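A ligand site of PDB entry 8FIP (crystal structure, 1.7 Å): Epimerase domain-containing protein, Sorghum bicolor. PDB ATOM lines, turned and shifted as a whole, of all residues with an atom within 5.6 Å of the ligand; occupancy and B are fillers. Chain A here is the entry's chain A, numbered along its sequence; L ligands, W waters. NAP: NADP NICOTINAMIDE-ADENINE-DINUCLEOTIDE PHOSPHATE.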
ATOM      1  N   THR A  17      10.983 -14.899   6.841  1.00  0.00           N
ATOM      2  CA  THR A  17      11.590 -16.072   6.220  1.00  0.00           C
ATOM      3  C   THR A  17      13.065 -16.210   6.625  1.00  0.00           C
ATOM      4  O   THR A  17      13.802 -15.232   6.615  1.00  0.00           O
ATOM      5  CB  THR A  17      11.509 -16.018   4.693  1.00  0.00           C
ATOM      6  OG1 THR A  17      12.183 -14.837   4.201  1.00  0.00           O
ATOM      7  CG2 THR A  17      10.021 -16.025   4.268  1.00  0.00           C
ATOM      8  N   GLY A  18      13.466 -17.419   6.973  1.00  0.00           N
ATOM      9  CA  GLY A  18      14.841 -17.716   7.323  1.00  0.00           C
ATOM     10  C   GLY A  18      15.164 -17.366   8.761  1.00  0.00           C
ATOM     11  O   GLY A  18      16.068 -16.569   9.011  1.00  0.00           O
ATOM     12  N   GLY A  19      14.488 -18.010   9.719  1.00  0.00           N
ATOM     13  CA  GLY A  19      14.612 -17.622  11.119  1.00  0.00           C
ATOM     14  C   GLY A  19      15.937 -17.958  11.766  1.00  0.00           C
ATOM     15  O   GLY A  19      16.230 -17.432  12.849  1.00  0.00           O
ATOM     16  N   ASN A  20      16.739 -18.815  11.148  1.00  0.00           N
ATOM     17  CA  ASN A  20      18.085 -19.129  11.620  1.00  0.00           C
ATOM     18  C   ASN A  20      19.131 -18.159  11.108  1.00  0.00           C
ATOM     19  O   ASN A  20      20.265 -18.185  11.606  1.00  0.00           O
ATOM     20  CB  ASN A  20      18.464 -20.540  11.177  1.00  0.00           C
ATOM     21  CG  ASN A  20      18.606 -20.645   9.661  1.00  0.00           C
ATOM     22  OD1 ASN A  20      17.617 -20.530   8.943  1.00  0.00           O
ATOM     23  ND2 ASN A  20      19.802 -20.921   9.183  1.00  0.00           N
ATOM     24  N   GLY A  21      18.791 -17.356  10.109  1.00  0.00           N
ATOM     25  CA  GLY A  21      19.750 -16.438   9.551  1.00  0.00           C
ATOM     26  C   GLY A  21      20.077 -15.312  10.521  1.00  0.00           C
ATOM     27  O   GLY A  21      19.342 -15.055  11.471  1.00  0.00           O
ATOM     28  N   TYR A  22      21.191 -14.647  10.258  1.00  0.00           N
ATOM     29  CA  TYR A  22      21.628 -13.507  11.082  1.00  0.00           C
ATOM     30  C   TYR A  22      20.539 -12.425  11.182  1.00  0.00           C
ATOM     31  O   TYR A  22      20.002 -12.166  12.256  1.00  0.00           O
ATOM     32  CB  TYR A  22      22.922 -12.978  10.468  1.00  0.00           C
ATOM     33  CG  TYR A  22      23.391 -11.665  11.028  1.00  0.00           C
ATOM     34  CD1 TYR A  22      23.509 -11.475  12.410  1.00  0.00           C
ATOM     35  CD2 TYR A  22      23.687 -10.613  10.189  1.00  0.00           C
ATOM     36  CE1 TYR A  22      23.954 -10.248  12.927  1.00  0.00           C
ATOM     37  CE2 TYR A  22      24.132  -9.405  10.679  1.00  0.00           C
ATOM     38  CZ  TYR A  22      24.245  -9.227  12.055  1.00  0.00           C
ATOM     39  OH  TYR A  22      24.674  -7.996  12.542  1.00  0.00           O
ATOM     40  N   ILE A  23      20.211 -11.778  10.050  1.00  0.00           N
ATOM     41  CA  ILE A  23      19.217 -10.710  10.072  1.00  0.00           C
ATOM     42  C   ILE A  23      17.837 -11.248  10.455  1.00  0.00           C
ATOM     43  O   ILE A  23      17.107 -10.600  11.228  1.00  0.00           O
ATOM     44  CB  ILE A  23      19.174  -9.995   8.705  1.00  0.00           C
ATOM     45  CG1 ILE A  23      20.483  -9.236   8.487  1.00  0.00           C
ATOM     46  CG2 ILE A  23      17.932  -9.040   8.660  1.00  0.00           C
ATOM     47  CD1 ILE A  23      20.693  -8.763   7.036  1.00  0.00           C
ATOM     48  N   GLY A  24      17.458 -12.401   9.909  1.00  0.00           N
ATOM     49  CA  GLY A  24      16.152 -12.973  10.236  1.00  0.00           C
ATOM     50  C   GLY A  24      15.965 -13.167  11.731  1.00  0.00           C
ATOM     51  O   GLY A  24      14.913 -12.809  12.283  1.00  0.00           O
ATOM     52  N   ARG A  43      14.565 -24.112   7.051  1.00  0.00           N
ATOM     53  CA  ARG A  43      14.545 -25.269   6.170  1.00  0.00           C
ATOM     54  C   ARG A  43      14.529 -26.596   6.937  1.00  0.00           C
ATOM     55  O   ARG A  43      14.065 -27.601   6.397  1.00  0.00           O
ATOM     56  CB  ARG A  43      15.723 -25.222   5.207  1.00  0.00           C
ATOM     57  CG  ARG A  43      15.576 -24.082   4.174  1.00  0.00           C
ATOM     58  CD  ARG A  43      16.316 -24.377   2.866  1.00  0.00           C
ATOM     59  NE  ARG A  43      17.704 -23.949   2.890  1.00  0.00           N
ATOM     60  CZ  ARG A  43      18.519 -23.996   1.846  1.00  0.00           C
ATOM     61  NH1 ARG A  43      18.146 -24.570   0.703  1.00  0.00           N
ATOM     62  NH2 ARG A  43      19.742 -23.490   1.941  1.00  0.00           N
ATOM     63  N   LYS A  50      21.576 -25.003  14.024  1.00  0.00           N
ATOM     64  CA  LYS A  50      21.139 -23.730  13.430  1.00  0.00           C
ATOM     65  C   LYS A  50      19.994 -23.070  14.185  1.00  0.00           C
ATOM     66  O   LYS A  50      19.870 -21.842  14.148  1.00  0.00           O
ATOM     67  CB  LYS A  50      20.698 -23.963  11.984  1.00  0.00           C
ATOM     68  CG  LYS A  50      21.895 -24.144  11.058  1.00  0.00           C
ATOM     69  CD  LYS A  50      21.466 -24.154   9.579  1.00  0.00           C
ATOM     70  CE  LYS A  50      22.658 -23.970   8.648  1.00  0.00           C
ATOM     71  NZ  LYS A  50      22.150 -24.049   7.234  1.00  0.00           N
ATOM     72  N   ALA A  68      10.129 -24.769   5.501  1.00  0.00           N
ATOM     73  CA  ALA A  68       9.925 -24.385   4.113  1.00  0.00           C
ATOM     74  C   ALA A  68      11.265 -24.101   3.435  1.00  0.00           C
ATOM     75  O   ALA A  68      12.192 -23.550   4.050  1.00  0.00           O
ATOM     76  CB  ALA A  68       9.019 -23.149   3.985  1.00  0.00           C
ATOM     77  N   ASP A  69      11.372 -24.483   2.158  1.00  0.00           N
ATOM     78  CA  ASP A  69      12.465 -24.088   1.285  1.00  0.00           C
ATOM     79  C   ASP A  69      11.903 -23.135   0.246  1.00  0.00           C
ATOM     80  O   ASP A  69      11.027 -23.517  -0.540  1.00  0.00           O
ATOM     81  CB  ASP A  69      13.126 -25.322   0.643  1.00  0.00           C
ATOM     82  CG  ASP A  69      14.342 -24.963  -0.203  1.00  0.00           C
ATOM     83  OD1 ASP A  69      14.289 -23.955  -0.935  1.00  0.00           O
ATOM     84  OD2 ASP A  69      15.370 -25.682  -0.127  1.00  0.00           O
ATOM     85  N   MET A  70      12.403 -21.889   0.221  1.00  0.00           N
ATOM     86  CA  MET A  70      11.760 -20.886  -0.624  1.00  0.00           C
ATOM     87  C   MET A  70      11.903 -21.172  -2.101  1.00  0.00           C
ATOM     88  O   MET A  70      11.188 -20.546  -2.894  1.00  0.00           O
ATOM     89  CB  MET A  70      12.268 -19.462  -0.312  1.00  0.00           C
ATOM     90  CG  MET A  70      12.165 -19.151   1.168  1.00  0.00           C
ATOM     91  SD  MET A  70      10.438 -18.645   1.503  1.00  0.00           S
ATOM     92  CE  MET A  70       9.987 -20.139   2.437  1.00  0.00           C
ATOM     93  N   ASP A  71      12.774 -22.082  -2.487  1.00  0.00           N
ATOM     94  CA  ASP A  71      12.969 -22.437  -3.884  1.00  0.00           C
ATOM     95  C   ASP A  71      11.802 -23.213  -4.482  1.00  0.00           C
ATOM     96  O   ASP A  71      11.683 -23.257  -5.721  1.00  0.00           O
ATOM     97  CB  ASP A  71      14.224 -23.293  -4.044  1.00  0.00           C
ATOM     98  CG  ASP A  71      14.586 -23.530  -5.503  1.00  0.00           C
ATOM     99  OD1 ASP A  71      14.948 -22.537  -6.161  1.00  0.00           O
ATOM    100  OD2 ASP A  71      14.515 -24.693  -5.988  1.00  0.00           O
ATOM    101  N   VAL A  89      13.417 -12.075   4.103  1.00  0.00           N
ATOM    102  CA  VAL A  89      14.830 -11.940   4.418  1.00  0.00           C
ATOM    103  C   VAL A  89      15.643 -13.052   3.782  1.00  0.00           C
ATOM    104  O   VAL A  89      16.674 -12.808   3.154  1.00  0.00           O
ATOM    105  CB  VAL A  89      15.021 -11.916   5.954  1.00  0.00           C
ATOM    106  CG1 VAL A  89      16.506 -11.768   6.287  1.00  0.00           C
ATOM    107  CG2 VAL A  89      14.198 -10.768   6.594  1.00  0.00           C
ATOM    108  N   ALA A  90      15.176 -14.290   3.946  1.00  0.00           N
ATOM    109  CA  ALA A  90      15.907 -15.422   3.394  1.00  0.00           C
ATOM    110  C   ALA A  90      16.145 -15.229   1.895  1.00  0.00           C
ATOM    111  O   ALA A  90      15.256 -14.757   1.176  1.00  0.00           O
ATOM    112  CB  ALA A  90      15.139 -16.727   3.625  1.00  0.00           C
ATOM    113  N   ALA A  91      17.317 -15.645   1.431  1.00  0.00           N
ATOM    114  CA  ALA A  91      17.651 -15.629   0.007  1.00  0.00           C
ATOM    115  C   ALA A  91      18.933 -16.388  -0.199  1.00  0.00           C
ATOM    116  O   ALA A  91      19.737 -16.542   0.737  1.00  0.00           O
ATOM    117  CB  ALA A  91      17.833 -14.201  -0.525  1.00  0.00           C
ATOM    118  N   PRO A  92      19.183 -16.835  -1.425  1.00  0.00           N
ATOM    119  CA  PRO A  92      20.454 -17.484  -1.724  1.00  0.00           C
ATOM    120  C   PRO A  92      21.595 -16.497  -1.501  1.00  0.00           C
ATOM    121  O   PRO A  92      21.510 -15.336  -1.899  1.00  0.00           O
ATOM    122  CB  PRO A  92      20.314 -17.865  -3.207  1.00  0.00           C
ATOM    123  CG  PRO A  92      18.855 -17.905  -3.459  1.00  0.00           C
ATOM    124  CD  PRO A  92      18.247 -16.876  -2.570  1.00  0.00           C
ATOM    125  N   VAL A  93      22.658 -16.975  -0.855  1.00  0.00           N
ATOM    126  CA  VAL A  93      23.787 -16.109  -0.584  1.00  0.00           C
ATOM    127  C   VAL A  93      25.067 -16.814  -1.010  1.00  0.00           C
ATOM    128  O   VAL A  93      26.046 -16.873  -0.261  1.00  0.00           O
ATOM    129  CB  VAL A  93      23.805 -15.671   0.899  1.00  0.00           C
ATOM    130  CG1 VAL A  93      22.731 -14.673   1.170  1.00  0.00           C
ATOM    131  CG2 VAL A  93      23.563 -16.911   1.786  1.00  0.00           C
ATOM    132  N   THR A 131      14.027  -7.761   1.755  1.00  0.00           N
ATOM    133  CA  THR A 131      15.417  -7.410   2.028  1.00  0.00           C
ATOM    134  C   THR A 131      16.255  -7.777   0.818  1.00  0.00           C
ATOM    135  O   THR A 131      16.422  -8.957   0.515  1.00  0.00           O
ATOM    136  CB  THR A 131      15.951  -8.100   3.282  1.00  0.00           C
ATOM    137  OG1 THR A 131      15.106  -7.755   4.392  1.00  0.00           O
ATOM    138  CG2 THR A 131      17.423  -7.621   3.569  1.00  0.00           C
ATOM    139  N   SER A 132      16.749  -6.771   0.116  1.00  0.00           N
ATOM    140  CA  SER A 132      17.728  -6.943  -0.942  1.00  0.00           C
ATOM    141  C   SER A 132      19.108  -6.563  -0.372  1.00  0.00           C
ATOM    142  O   SER A 132      19.389  -6.902   0.785  1.00  0.00           O
ATOM    143  CB  SER A 132      17.367  -6.107  -2.171  1.00  0.00           C
ATOM    144  OG  SER A 132      18.319  -6.277  -3.211  1.00  0.00           O
ATOM    145  N   SER A 133      19.942  -5.885  -1.139  1.00  0.00           N
ATOM    146  CA  SER A 133      21.256  -5.495  -0.638  1.00  0.00           C
ATOM    147  C   SER A 133      21.750  -4.267  -1.381  1.00  0.00           C
ATOM    148  O   SER A 133      21.392  -4.044  -2.547  1.00  0.00           O
ATOM    149  CB  SER A 133      22.267  -6.641  -0.816  1.00  0.00           C
ATOM    150  OG  SER A 133      23.584  -6.176  -0.630  1.00  0.00           O
ATOM    151  N   ALA A 134      22.644  -3.523  -0.724  1.00  0.00           N
ATOM    152  CA  ALA A 134      23.415  -2.492  -1.408  1.00  0.00           C
ATOM    153  C   ALA A 134      24.158  -3.030  -2.638  1.00  0.00           C
ATOM    154  O   ALA A 134      24.464  -2.237  -3.537  1.00  0.00           O
ATOM    155  CB  ALA A 134      24.465  -1.884  -0.457  1.00  0.00           C
ATOM    156  N   TYR A 171      26.193 -12.428  -7.221  1.00  0.00           N
ATOM    157  CA  TYR A 171      25.408 -11.909  -6.102  1.00  0.00           C
ATOM    158  C   TYR A 171      24.834 -10.540  -6.433  1.00  0.00           C
ATOM    159  O   TYR A 171      23.646 -10.283  -6.223  1.00  0.00           O
ATOM    160  CB  TYR A 171      26.280 -11.833  -4.862  1.00  0.00           C
ATOM    161  CG  TYR A 171      25.634 -11.364  -3.587  1.00  0.00           C
ATOM    162  CD1 TYR A 171      24.737 -12.164  -2.897  1.00  0.00           C
ATOM    163  CD2 TYR A 171      25.975 -10.125  -3.032  1.00  0.00           C
ATOM    164  CE1 TYR A 171      24.148 -11.741  -1.692  1.00  0.00           C
ATOM    165  CE2 TYR A 171      25.405  -9.691  -1.846  1.00  0.00           C
ATOM    166  CZ  TYR A 171      24.523 -10.508  -1.167  1.00  0.00           C
ATOM    167  OH  TYR A 171      23.983 -10.053   0.036  1.00  0.00           O
ATOM    168  N   LYS A 175      20.655  -9.551  -7.073  1.00  0.00           N
ATOM    169  CA  LYS A 175      19.841  -8.592  -6.351  1.00  0.00           C
ATOM    170  C   LYS A 175      19.098  -7.671  -7.305  1.00  0.00           C
ATOM    171  O   LYS A 175      17.921  -7.374  -7.098  1.00  0.00           O
ATOM    172  CB  LYS A 175      20.710  -7.770  -5.383  1.00  0.00           C
ATOM    173  CG  LYS A 175      21.235  -8.552  -4.154  1.00  0.00           C
ATOM    174  CD  LYS A 175      20.218  -9.536  -3.538  1.00  0.00           C
ATOM    175  CE  LYS A 175      20.856 -10.176  -2.264  1.00  0.00           C
ATOM    176  NZ  LYS A 175      19.984 -11.199  -1.616  1.00  0.00           N
ATOM    177  N   CYS A 197      17.524  -2.027   0.919  1.00  0.00           N
ATOM    178  CA  CYS A 197      18.858  -2.406   0.472  1.00  0.00           C
ATOM    179  C   CYS A 197      19.896  -2.056   1.542  1.00  0.00           C
ATOM    180  O   CYS A 197      20.481  -0.958   1.512  1.00  0.00           O
ATOM    181  CB  CYS A 197      19.191  -1.683  -0.838  1.00  0.00           C
ATOM    182  SG  CYS A 197      18.064  -2.133  -2.189  1.00  0.00           S
ATOM    183  N   PRO A 198      20.146  -2.926   2.511  1.00  0.00           N
ATOM    184  CA  PRO A 198      21.121  -2.585   3.549  1.00  0.00           C
ATOM    185  C   PRO A 198      22.545  -2.736   3.033  1.00  0.00           C
ATOM    186  O   PRO A 198      22.819  -3.486   2.101  1.00  0.00           O
ATOM    187  CB  PRO A 198      20.796  -3.561   4.689  1.00  0.00           C
ATOM    188  CG  PRO A 198      20.050  -4.696   4.043  1.00  0.00           C
ATOM    189  CD  PRO A 198      19.446  -4.210   2.780  1.00  0.00           C
ATOM    190  N   VAL A 199      23.448  -1.966   3.647  1.00  0.00           N
ATOM    191  CA  VAL A 199      24.885  -2.148   3.460  1.00  0.00           C
ATOM    192  C   VAL A 199      25.368  -3.203   4.465  1.00  0.00           C
ATOM    193  O   VAL A 199      24.558  -3.859   5.121  1.00  0.00           O
ATOM    194  CB  VAL A 199      25.618  -0.809   3.653  1.00  0.00           C
ATOM    195  CG1 VAL A 199      25.183   0.170   2.579  1.00  0.00           C
ATOM    196  CG2 VAL A 199      25.345  -0.236   5.045  1.00  0.00           C
ATOM    197  N   LEU A 200      26.687  -3.372   4.591  1.00  0.00           N
ATOM    198  CA  LEU A 200      27.237  -4.378   5.497  1.00  0.00           C
ATOM    199  C   LEU A 200      26.693  -4.143   6.904  1.00  0.00           C
ATOM    200  O   LEU A 200      26.779  -3.034   7.431  1.00  0.00           O
ATOM    201  CB  LEU A 200      28.763  -4.343   5.492  1.00  0.00           C
ATOM    202  CG  LEU A 200      29.501  -5.481   6.217  1.00  0.00           C
ATOM    203  CD1 LEU A 200      29.373  -6.782   5.453  1.00  0.00           C
ATOM    204  CD2 LEU A 200      30.983  -5.117   6.457  1.00  0.00           C
ATOM    205  N   THR A 201      26.130  -5.193   7.498  1.00  0.00           N
ATOM    206  CA  THR A 201      25.367  -5.086   8.747  1.00  0.00           C
ATOM    207  C   THR A 201      26.158  -5.690   9.901  1.00  0.00           C
ATOM    208  O   THR A 201      26.722  -6.779   9.787  1.00  0.00           O
ATOM    209  CB  THR A 201      24.010  -5.792   8.587  1.00  0.00           C
ATOM    210  OG1 THR A 201      23.295  -5.186   7.485  1.00  0.00           O
ATOM    211  CG2 THR A 201      23.149  -5.639   9.820  1.00  0.00           C
ATOM    212  N   VAL A 210      26.025 -18.373  12.626  1.00  0.00           N
ATOM    213  CA  VAL A 210      26.071 -17.527  11.445  1.00  0.00           C
ATOM    214  C   VAL A 210      27.511 -17.126  11.169  1.00  0.00           C
ATOM    215  O   VAL A 210      28.371 -17.175  12.037  1.00  0.00           O
ATOM    216  CB  VAL A 210      25.175 -16.285  11.593  1.00  0.00           C
ATOM    217  CG1 VAL A 210      23.756 -16.707  11.945  1.00  0.00           C
ATOM    218  CG2 VAL A 210      25.754 -15.346  12.637  1.00  0.00           C
ATOM    219  N   ARG A 211      27.750 -16.778   9.906  1.00  0.00           N
ATOM    220  CA  ARG A 211      29.034 -16.220   9.492  1.00  0.00           C
ATOM    221  C   ARG A 211      28.803 -14.853   8.854  1.00  0.00           C
ATOM    222  O   ARG A 211      28.943 -13.823   9.528  1.00  0.00           O
ATOM    223  CB  ARG A 211      29.740 -17.185   8.534  1.00  0.00           C
ATOM    224  CG  ARG A 211      30.176 -18.463   9.270  1.00  0.00           C
ATOM    225  CD  ARG A 211      30.981 -19.401   8.382  1.00  0.00           C
ATOM    226  NE  ARG A 211      32.402 -19.256   8.670  1.00  0.00           N
ATOM    227  CZ  ARG A 211      33.287 -18.700   7.858  1.00  0.00           C
ATOM    228  NH1 ARG A 211      32.953 -18.248   6.653  1.00  0.00           N
ATOM    229  NH2 ARG A 211      34.545 -18.597   8.271  1.00  0.00           N
ATOM    230  N   THR A 212      28.423 -14.849   7.572  1.00  0.00           N
ATOM    231  CA  THR A 212      27.958 -13.655   6.857  1.00  0.00           C
ATOM    232  C   THR A 212      28.771 -12.409   7.236  1.00  0.00           C
ATOM    233  O   THR A 212      30.007 -12.477   7.293  1.00  0.00           O
ATOM    234  CB  THR A 212      26.439 -13.473   7.059  1.00  0.00           C
ATOM    235  OG1 THR A 212      25.943 -12.346   6.286  1.00  0.00           O
ATOM    236  CG2 THR A 212      26.027 -13.317   8.534  1.00  0.00           C
ATOM    237  N   SER A 213      28.093 -11.282   7.459  1.00  0.00           N
ATOM    238  CA  SER A 213      28.777 -10.012   7.707  1.00  0.00           C
ATOM    239  C   SER A 213      29.471  -9.961   9.084  1.00  0.00           C
ATOM    240  O   SER A 213      30.238  -9.015   9.345  1.00  0.00           O
ATOM    241  CB  SER A 213      27.785  -8.860   7.629  1.00  0.00           C
ATOM    242  OG  SER A 213      26.647  -9.145   8.452  1.00  0.00           O
HETATM  243  PA  NAP L   1      22.703 -15.675   6.662  1.00  0.00           P
HETATM  244  O1A NAP L   1      22.968 -15.718   8.141  1.00  0.00           O
HETATM  245  O2A NAP L   1      23.673 -16.550   5.869  1.00  0.00           O
HETATM  246  O5B NAP L   1      21.137 -16.026   6.411  1.00  0.00           O
HETATM  247  C5B NAP L   1      20.718 -16.473   5.138  1.00  0.00           C
HETATM  248  C4B NAP L   1      19.272 -16.981   5.381  1.00  0.00           C
HETATM  249  O4B NAP L   1      18.702 -17.258   4.171  1.00  0.00           O
HETATM  250  C3B NAP L   1      19.259 -18.286   6.184  1.00  0.00           C
HETATM  251  O3B NAP L   1      18.167 -18.325   7.000  1.00  0.00           O
HETATM  252  C2B NAP L   1      19.166 -19.307   4.996  1.00  0.00           C
HETATM  253  O2B NAP L   1      18.694 -20.603   5.491  1.00  0.00           O
HETATM  254  C1B NAP L   1      18.234 -18.743   4.209  1.00  0.00           C
HETATM  255  N9A NAP L   1      18.112 -19.335   2.877  1.00  0.00           N
HETATM  256  C8A NAP L   1      18.988 -19.382   1.869  1.00  0.00           C
HETATM  257  N7A NAP L   1      18.422 -20.075   0.861  1.00  0.00           N
HETATM  258  C5A NAP L   1      17.193 -20.480   1.280  1.00  0.00           C
HETATM  259  C6A NAP L   1      16.182 -21.214   0.709  1.00  0.00           C
HETATM  260  N6A NAP L   1      16.255 -21.764  -0.607  1.00  0.00           N
HETATM  261  N1A NAP L   1      15.052 -21.451   1.365  1.00  0.00           N
HETATM  262  C2A NAP L   1      14.900 -20.974   2.608  1.00  0.00           C
HETATM  263  N3A NAP L   1      15.874 -20.263   3.185  1.00  0.00           N
HETATM  264  C4A NAP L   1      17.007 -20.008   2.523  1.00  0.00           C
HETATM  265  O3  NAP L   1      22.932 -14.192   6.036  1.00  0.00           O
HETATM  266  PN  NAP L   1      22.182 -12.792   6.355  1.00  0.00           P
HETATM  267  O1N NAP L   1      23.313 -11.808   6.344  1.00  0.00           O
HETATM  268  O2N NAP L   1      21.288 -12.806   7.549  1.00  0.00           O
HETATM  269  O5D NAP L   1      21.276 -12.666   4.993  1.00  0.00           O
HETATM  270  C5D NAP L   1      19.908 -12.409   5.063  1.00  0.00           C
HETATM  271  C4D NAP L   1      19.589 -11.622   3.748  1.00  0.00           C
HETATM  272  O4D NAP L   1      20.078 -10.173   3.994  1.00  0.00           O
HETATM  273  C3D NAP L   1      20.214 -12.000   2.692  1.00  0.00           C
HETATM  274  O3D NAP L   1      19.284 -11.896   1.537  1.00  0.00           O
HETATM  275  C2D NAP L   1      21.405 -10.935   2.326  1.00  0.00           C
HETATM  276  O2D NAP L   1      21.559 -10.817   0.873  1.00  0.00           O
HETATM  277  C1D NAP L   1      20.868  -9.851   2.757  1.00  0.00           C
HETATM  278  N1N NAP L   1      21.867  -8.833   3.208  1.00  0.00           N
HETATM  279  C2N NAP L   1      22.771  -9.076   4.226  1.00  0.00           C
HETATM  280  C3N NAP L   1      23.669  -8.058   4.556  1.00  0.00           C
HETATM  281  C7N NAP L   1      24.707  -8.229   5.708  1.00  0.00           C
HETATM  282  O7N NAP L   1      25.602  -7.421   5.860  1.00  0.00           O
HETATM  283  N7N NAP L   1      24.544  -9.354   6.570  1.00  0.00           N
HETATM  284  C4N NAP L   1      23.660  -6.861   3.931  1.00  0.00           C
HETATM  285  C5N NAP L   1      22.756  -6.634   2.928  1.00  0.00           C
HETATM  286  C6N NAP L   1      21.852  -7.657   2.580  1.00  0.00           C
HETATM  287  P2B NAP L   1      19.705 -21.909   5.413  1.00  0.00           P
HETATM  288  O1X NAP L   1      18.843 -23.176   5.509  1.00  0.00           O
HETATM  289  O2X NAP L   1      20.513 -21.865   4.129  1.00  0.00           O
HETATM  290  O3X NAP L   1      20.651 -21.851   6.582  1.00  0.00           O
HETATM  291  O   HOH W   1      25.655 -17.301   7.927  1.00  0.00           O
HETATM  292  O   HOH W   2      16.737 -15.086   6.695  1.00  0.00           O
HETATM  293  O   HOH W   3      15.332 -20.731   6.000  1.00  0.00           O
HETATM  294  O   HOH W   4      16.991 -22.576   7.402  1.00  0.00           O
HETATM  295  O   HOH W   5      25.029  -7.826   0.998  1.00  0.00           O
HETATM  296  O   HOH W   6      22.918 -20.456   6.869  1.00  0.00           O
HETATM  297  O   HOH W   7      18.810 -13.829   7.945  1.00  0.00           O
HETATM  298  O   HOH W   8      22.711 -23.469   4.036  1.00  0.00           O
HETATM  299  O   HOH W   9      17.702 -21.406  -3.178  1.00  0.00           O
HETATM  300  O   HOH W  10      19.696 -25.524   6.257  1.00  0.00           O
HETATM  301  O   HOH W  11      22.044 -20.020   2.749  1.00  0.00           O
HETATM  302  O   HOH W  12      23.665 -18.976   4.714  1.00  0.00           O
HETATM  303  O   HOH W  13      22.835 -18.322   8.880  1.00  0.00           O
HETATM  304  O   HOH W  14      12.620 -21.110   5.117  1.00  0.00           O
HETATM  305  O   HOH W  15      15.332 -19.386  -2.565  1.00  0.00           O
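The side-chain hydroxyl of Tyr 171 is in hydrogen-bond range of an oxygen (O2D) of the ligand (2.7 Å).
An oxygen (O1N) of the ligand is in hydrogen-bond range of the side-chain hydroxyl of Thr 212, at 2.7 Å.
NZ of Lys 50 is in salt-bridge range of O3X of the ligand, at 2.7 Å.
O7N of the ligand is in hydrogen-bond range of N of Thr 201 (2.8 Å).
N7N of the ligand is in hydrogen-bond range of OG of Ser 213, at 2.8 Å.
An oxygen (O2X) of the ligand lies within salt-bridge range of the guanidinium group of Arg 43 (2.8 Å).
An oxygen (O3X) of the ligand is in hydrogen-bond range of the side-chain amide nitrogen (ND2) of Asn 20 (2.9 Å).
N of Ile 23 sits at hydrogen-bond distance from O2N of the ligand, 2.9 Å away.
The backbone NH (N) of Met 70 lies within hydrogen-bond range of a nitrogen (N1A) of the ligand (2.9 Å).
A nitrogen (N6A) of the ligand is in hydrogen-bond range of the side-chain carboxylate of Asp 69 (3.0 Å).
The backbone NH (N) of Tyr 22 is in hydrogen-bond range of an oxygen (O1A) of the ligand (3.0 Å).
The side-chain amino group of Lys 175 sits at hydrogen-bond distance from an oxygen (O2D) of the ligand.
The backbone NH (N) of Ala 91 lies within hydrogen-bond range of an oxygen (O4B) of the ligand, at 3.5 Å.
The backbone carbonyl oxygen (O) of Val 89 lies close to an oxygen (O3D) of the ligand (3.2 Å).
O3B of the ligand sits at hydrogen-bond distance from N of Gly 21 (3.3 Å).
An oxygen (O3B) of the ligand sits at hydrogen-bond distance from the backbone carbonyl oxygen (O) of Gly 18 (3.4 Å).
The side-chain hydroxyl (OG) of Ser 213 is in hydrogen-bond range of the backbone carbonyl oxygen (O) of Thr 201, 2.7 Å away.
The side-chain hydroxyl (OG1) of Thr 201 lies within hydrogen-bond range of the backbone carbonyl oxygen (O) of Val 199, 3.0 Å away.
The guanidinium group (NH1) of Arg 43 lies within salt-bridge range of the side-chain carboxylate (OD2) of Asp 69 (3.1 Å).
N of Asp 71 is in hydrogen-bond range of OD1 of Asp 69, 2.9 Å away.
N of Val 89 lies within hydrogen-bond range of OG1 of Thr 17.
O of Pro 198 lies within hydrogen-bond range of N of Ala 134 (2.8 Å).
The backbone NH (N) of Ala 90 sits at hydrogen-bond distance from the side-chain hydroxyl (OG1) of Thr 17, at 3.1 Å.
Asp 71 touches the ligand.
Ala 90 touches the ligand.
Val 93 touches the ligand.
Thr 131 touches the ligand.
Ser 132 touches the ligand (O to C6N, 3.1 Å).
Ser 133 touches the ligand (CB to C6N, 3.6 Å).
O of Pro 198 touches C5N of the ligand, at 3.3 Å.
O of Val 199 touches C4N of the ligand, at 3.4 Å.
Leu 200 touches the ligand (CA to O7N, 3.5 Å).
Hydrophobic or aromatic side chains within 4 Å of the ligand: Tyr 22, Ile 23, Met 70, Val 89, Ala 90, Ala 91, Val 93, Tyr 171, Pro 198 and Leu 200.
25 residues have an atom within 4 Å of the ligand: Gly 18, Asn 20, Gly 21, Tyr 22, Ile 23, Arg 43, Lys 50, Asp 69, Met 70, Asp 71, Val 89, Ala 90, Ala 91, Val 93, Thr 131, Ser 132, Ser 133, Tyr 171, Lys 175, Pro 198, Val 199, Leu 200, Thr 201, Thr 212 and Ser 213.
Water W10 bridges an oxygen (O1X) of the ligand (2.6 Å) and the side-chain amino group (NZ) of Lys 50 (3.0 Å).
Water W4 lies within hydrogen-bond range of the side-chain amide oxygen (OD1) of Asn 20 (2.6 Å), an oxygen (O1X) of the ligand (2.7 Å) and the backbone NH (N) of Arg 43 (2.9 Å).
Water W8 lies within hydrogen-bond range of O2X of the ligand and NZ of Lys 50.
Water W1 bridges N of Arg 211 (2.9 Å) and O2A of the ligand (3.0 Å).
Water W5 bridges the side-chain hydroxyl (OH) of Tyr 171 (2.6 Å) and the side-chain hydroxyl (OG) of Ser 133 (2.7 Å).
Water W2 lies within hydrogen-bond range of O of Gly 18 (2.8 Å), O of Thr 17 (2.9 Å) and N of Ala 90 (3.3 Å).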
